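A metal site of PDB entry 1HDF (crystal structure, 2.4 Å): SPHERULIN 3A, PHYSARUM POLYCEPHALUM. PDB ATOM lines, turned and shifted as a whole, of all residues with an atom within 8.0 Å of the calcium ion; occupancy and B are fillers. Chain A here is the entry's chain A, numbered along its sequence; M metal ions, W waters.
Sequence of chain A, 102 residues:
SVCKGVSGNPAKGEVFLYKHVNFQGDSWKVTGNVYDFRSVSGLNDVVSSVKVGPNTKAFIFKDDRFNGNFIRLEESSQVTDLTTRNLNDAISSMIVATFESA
Four residues have an atom within 4 Å of the calcium ion: Asp 45, Lys 62, Ala 90 and Ser 92.
The side-chain hydroxyl (OG) of Ser 92 lies close to the side-chain amide nitrogen (ND2) of Asn 44, 2.7 Å away.
O of Phe 61 is in hydrogen-bond range of N of Ser 92 (2.8 Å).
The backbone carbonyl oxygen of Ser 92 sits at hydrogen-bond distance from the backbone NH of Phe 37, 2.9 Å away.
The backbone NH (N) of Asp 45 lies within hydrogen-bond range of the backbone carbonyl oxygen (O) of Ile 91 (3.2 Å).
ND2 of Asn 44 lies close to OD1 of Asp 45, at 3.5 Å.
The calcium ion is bound by O of Lys 62 (2.4 Å), OG of Ser 92 (2.4 Å), O of Ala 90 (2.4 Å), OD1 of Asp 45 (2.5 Å), water W3 (2.6 Å), water W2 (2.7 Å) and water W1 (2.8 Å).
The calcium ion has seven donor atoms within binding distance.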
ATOM      1  N   PHE A  37       6.805   5.702 -11.346  1.00  0.00           N
ATOM      2  CA  PHE A  37       5.981   4.524 -11.102  1.00  0.00           C
ATOM      3  C   PHE A  37       6.402   3.804  -9.827  1.00  0.00           C
ATOM      4  O   PHE A  37       5.705   2.893  -9.349  1.00  0.00           O
ATOM      5  CB  PHE A  37       6.048   3.585 -12.312  1.00  0.00           C
ATOM      6  CG  PHE A  37       5.113   3.947 -13.422  1.00  0.00           C
ATOM      7  CD1 PHE A  37       4.750   5.273 -13.641  1.00  0.00           C
ATOM      8  CD2 PHE A  37       4.594   2.965 -14.241  1.00  0.00           C
ATOM      9  CE1 PHE A  37       3.873   5.606 -14.676  1.00  0.00           C
ATOM     10  CE2 PHE A  37       3.711   3.286 -15.283  1.00  0.00           C
ATOM     11  CZ  PHE A  37       3.348   4.614 -15.487  1.00  0.00           C
ATOM     12  N   ARG A  38       7.539   4.207  -9.283  1.00  0.00           N
ATOM     13  CA  ARG A  38       8.071   3.627  -8.062  1.00  0.00           C
ATOM     14  C   ARG A  38       7.231   4.042  -6.861  1.00  0.00           C
ATOM     15  O   ARG A  38       7.294   3.421  -5.799  1.00  0.00           O
ATOM     16  CB  ARG A  38       9.503   4.088  -7.830  1.00  0.00           C
ATOM     17  CG  ARG A  38      10.573   3.069  -8.082  1.00  0.00           C
ATOM     18  CD  ARG A  38      10.933   2.952  -9.521  1.00  0.00           C
ATOM     19  NE  ARG A  38      12.354   3.172  -9.731  1.00  0.00           N
ATOM     20  CZ  ARG A  38      12.957   4.347  -9.595  1.00  0.00           C
ATOM     21  NH1 ARG A  38      12.263   5.413  -9.249  1.00  0.00           N
ATOM     22  NH2 ARG A  38      14.265   4.454  -9.811  1.00  0.00           N
ATOM     23  N   ASN A  44       6.180  -0.193 -11.178  1.00  0.00           N
ATOM     24  CA  ASN A  44       7.361  -0.007 -12.007  1.00  0.00           C
ATOM     25  C   ASN A  44       7.805  -1.247 -12.774  1.00  0.00           C
ATOM     26  O   ASN A  44       7.834  -2.354 -12.239  1.00  0.00           O
ATOM     27  CB  ASN A  44       8.551   0.463 -11.169  1.00  0.00           C
ATOM     28  CG  ASN A  44       9.674   1.019 -12.023  1.00  0.00           C
ATOM     29  OD1 ASN A  44      10.858   0.843 -11.727  1.00  0.00           O
ATOM     30  ND2 ASN A  44       9.301   1.717 -13.096  1.00  0.00           N
ATOM     31  N   ASP A  45       8.140  -1.033 -14.043  1.00  0.00           N
ATOM     32  CA  ASP A  45       8.613  -2.078 -14.933  1.00  0.00           C
ATOM     33  C   ASP A  45       7.797  -3.363 -15.049  1.00  0.00           C
ATOM     34  O   ASP A  45       8.383  -4.426 -15.261  1.00  0.00           O
ATOM     35  CB  ASP A  45      10.058  -2.439 -14.561  1.00  0.00           C
ATOM     36  CG  ASP A  45      11.026  -1.289 -14.800  1.00  0.00           C
ATOM     37  OD1 ASP A  45      10.663  -0.353 -15.539  1.00  0.00           O
ATOM     38  OD2 ASP A  45      12.153  -1.328 -14.261  1.00  0.00           O
ATOM     39  N   VAL A  46       6.475  -3.298 -14.933  1.00  0.00           N
ATOM     40  CA  VAL A  46       5.655  -4.502 -15.077  1.00  0.00           C
ATOM     41  C   VAL A  46       4.525  -4.384 -16.091  1.00  0.00           C
ATOM     42  O   VAL A  46       3.904  -5.384 -16.441  1.00  0.00           O
ATOM     43  CB  VAL A  46       5.029  -4.966 -13.734  1.00  0.00           C
ATOM     44  CG1 VAL A  46       6.128  -5.084 -12.656  1.00  0.00           C
ATOM     45  CG2 VAL A  46       3.926  -4.009 -13.308  1.00  0.00           C
ATOM     46  N   PHE A  61       7.171   6.606 -20.559  1.00  0.00           N
ATOM     47  CA  PHE A  61       8.629   6.706 -20.574  1.00  0.00           C
ATOM     48  C   PHE A  61       9.325   5.512 -19.957  1.00  0.00           C
ATOM     49  O   PHE A  61       8.839   4.937 -18.986  1.00  0.00           O
ATOM     50  CB  PHE A  61       9.057   7.981 -19.838  1.00  0.00           C
ATOM     51  CG  PHE A  61       8.475   9.215 -20.414  1.00  0.00           C
ATOM     52  CD1 PHE A  61       7.113   9.493 -20.239  1.00  0.00           C
ATOM     53  CD2 PHE A  61       9.237  10.063 -21.213  1.00  0.00           C
ATOM     54  CE1 PHE A  61       6.530  10.582 -20.859  1.00  0.00           C
ATOM     55  CE2 PHE A  61       8.666  11.149 -21.840  1.00  0.00           C
ATOM     56  CZ  PHE A  61       7.310  11.414 -21.663  1.00  0.00           C
ATOM     57  N   LYS A  62      10.472   5.155 -20.519  1.00  0.00           N
ATOM     58  CA  LYS A  62      11.210   4.010 -20.012  1.00  0.00           C
ATOM     59  C   LYS A  62      11.761   4.271 -18.628  1.00  0.00           C
ATOM     60  O   LYS A  62      11.843   3.355 -17.810  1.00  0.00           O
ATOM     61  CB  LYS A  62      12.361   3.651 -20.943  1.00  0.00           C
ATOM     62  CG  LYS A  62      13.102   2.398 -20.520  1.00  0.00           C
ATOM     63  CD  LYS A  62      13.812   1.762 -21.697  1.00  0.00           C
ATOM     64  CE  LYS A  62      14.232   0.338 -21.377  1.00  0.00           C
ATOM     65  NZ  LYS A  62      14.942  -0.294 -22.511  1.00  0.00           N
ATOM     66  N   ASP A  63      12.136   5.519 -18.353  1.00  0.00           N
ATOM     67  CA  ASP A  63      12.684   5.879 -17.062  1.00  0.00           C
ATOM     68  C   ASP A  63      11.734   6.782 -16.288  1.00  0.00           C
ATOM     69  O   ASP A  63      10.715   7.237 -16.811  1.00  0.00           O
ATOM     70  CB  ASP A  63      14.036   6.572 -17.214  1.00  0.00           C
ATOM     71  CG  ASP A  63      15.052   5.719 -17.948  1.00  0.00           C
ATOM     72  OD1 ASP A  63      14.980   4.476 -17.808  1.00  0.00           O
ATOM     73  OD2 ASP A  63      15.928   6.271 -18.635  1.00  0.00           O
ATOM     74  N   ASP A  64      12.088   7.058 -15.042  1.00  0.00           N
ATOM     75  CA  ASP A  64      11.287   7.926 -14.192  1.00  0.00           C
ATOM     76  C   ASP A  64      11.533   9.378 -14.618  1.00  0.00           C
ATOM     77  O   ASP A  64      12.472   9.664 -15.373  1.00  0.00           O
ATOM     78  CB  ASP A  64      11.729   7.778 -12.739  1.00  0.00           C
ATOM     79  CG  ASP A  64      13.164   8.231 -12.528  1.00  0.00           C
ATOM     80  OD1 ASP A  64      14.066   7.590 -13.098  1.00  0.00           O
ATOM     81  OD2 ASP A  64      13.390   9.226 -11.801  1.00  0.00           O
ATOM     82  N   ASN A  67      12.231  10.545 -18.568  1.00  0.00           N
ATOM     83  CA  ASN A  67      13.504  10.411 -19.282  1.00  0.00           C
ATOM     84  C   ASN A  67      13.540   9.080 -20.019  1.00  0.00           C
ATOM     85  O   ASN A  67      12.697   8.213 -19.781  1.00  0.00           O
ATOM     86  CB  ASN A  67      14.680  10.458 -18.302  1.00  0.00           C
ATOM     87  CG  ASN A  67      14.752  11.770 -17.540  1.00  0.00           C
ATOM     88  OD1 ASN A  67      14.769  12.844 -18.143  1.00  0.00           O
ATOM     89  ND2 ASN A  67      14.811  11.685 -16.212  1.00  0.00           N
ATOM     90  N   LEU A  87       8.619  -1.476 -25.227  1.00  0.00           N
ATOM     91  CA  LEU A  87       8.431  -0.968 -23.867  1.00  0.00           C
ATOM     92  C   LEU A  87       7.750  -1.912 -22.896  1.00  0.00           C
ATOM     93  O   LEU A  87       7.045  -1.470 -21.986  1.00  0.00           O
ATOM     94  CB  LEU A  87       7.676   0.361 -23.915  1.00  0.00           C
ATOM     95  CG  LEU A  87       8.481   1.539 -24.478  1.00  0.00           C
ATOM     96  CD1 LEU A  87       7.593   2.769 -24.604  1.00  0.00           C
ATOM     97  CD2 LEU A  87       9.661   1.815 -23.575  1.00  0.00           C
ATOM     98  N   ASN A  88       7.942  -3.220 -23.072  1.00  0.00           N
ATOM     99  CA  ASN A  88       7.334  -4.185 -22.169  1.00  0.00           C
ATOM    100  C   ASN A  88       8.111  -4.186 -20.858  1.00  0.00           C
ATOM    101  O   ASN A  88       9.343  -4.094 -20.861  1.00  0.00           O
ATOM    102  CB  ASN A  88       7.358  -5.580 -22.794  1.00  0.00           C
ATOM    103  CG  ASN A  88       6.543  -6.602 -22.003  1.00  0.00           C
ATOM    104  OD1 ASN A  88       6.881  -7.785 -21.968  1.00  0.00           O
ATOM    105  ND2 ASN A  88       5.471  -6.141 -21.363  1.00  0.00           N
ATOM    106  N   ASP A  89       7.398  -4.273 -19.733  1.00  0.00           N
ATOM    107  CA  ASP A  89       8.021  -4.273 -18.403  1.00  0.00           C
ATOM    108  C   ASP A  89       9.156  -3.256 -18.295  1.00  0.00           C
ATOM    109  O   ASP A  89      10.247  -3.609 -17.865  1.00  0.00           O
ATOM    110  CB  ASP A  89       8.580  -5.663 -18.070  1.00  0.00           C
ATOM    111  CG  ASP A  89       7.522  -6.747 -18.100  1.00  0.00           C
ATOM    112  OD1 ASP A  89       6.356  -6.458 -17.767  1.00  0.00           O
ATOM    113  OD2 ASP A  89       7.861  -7.904 -18.450  1.00  0.00           O
ATOM    114  N   ALA A  90       8.905  -2.017 -18.660  1.00  0.00           N
ATOM    115  CA  ALA A  90       9.965  -1.007 -18.595  1.00  0.00           C
ATOM    116  C   ALA A  90       9.514   0.417 -18.341  1.00  0.00           C
ATOM    117  O   ALA A  90      10.352   1.295 -18.097  1.00  0.00           O
ATOM    118  CB  ALA A  90      10.785  -1.065 -19.869  1.00  0.00           C
ATOM    119  N   ILE A  91       8.206   0.661 -18.382  1.00  0.00           N
ATOM    120  CA  ILE A  91       7.691   2.006 -18.164  1.00  0.00           C
ATOM    121  C   ILE A  91       7.909   2.425 -16.720  1.00  0.00           C
ATOM    122  O   ILE A  91       7.641   1.657 -15.793  1.00  0.00           O
ATOM    123  CB  ILE A  91       6.197   2.090 -18.506  1.00  0.00           C
ATOM    124  CG1 ILE A  91       5.993   1.759 -19.993  1.00  0.00           C
ATOM    125  CG2 ILE A  91       5.660   3.487 -18.215  1.00  0.00           C
ATOM    126  CD1 ILE A  91       4.555   1.690 -20.421  1.00  0.00           C
ATOM    127  N   SER A  92       8.417   3.641 -16.518  1.00  0.00           N
ATOM    128  CA  SER A  92       8.692   4.123 -15.178  1.00  0.00           C
ATOM    129  C   SER A  92       8.097   5.502 -14.879  1.00  0.00           C
ATOM    130  O   SER A  92       8.273   6.019 -13.778  1.00  0.00           O
ATOM    131  CB  SER A  92      10.196   4.135 -14.936  1.00  0.00           C
ATOM    132  OG  SER A  92      10.740   2.824 -15.099  1.00  0.00           O
ATOM    133  N   SER A  93       7.404   6.087 -15.855  1.00  0.00           N
ATOM    134  CA  SER A  93       6.760   7.376 -15.684  1.00  0.00           C
ATOM    135  C   SER A  93       5.774   7.555 -16.836  1.00  0.00           C
ATOM    136  O   SER A  93       5.866   6.886 -17.864  1.00  0.00           O
ATOM    137  CB  SER A  93       7.774   8.534 -15.647  1.00  0.00           C
ATOM    138  OG  SER A  93       8.493   8.679 -16.848  1.00  0.00           O
HETATM  139 CA    CA M   1      12.139   1.458 -16.430  1.00  0.00          CA
HETATM  140  O   HOH W   1      13.847  -0.163 -17.912  1.00  0.00           O
HETATM  141  O   HOH W   2      14.520   2.725 -15.934  1.00  0.00           O
HETATM  142  O   HOH W   3      13.548   1.101 -14.234  1.00  0.00           O
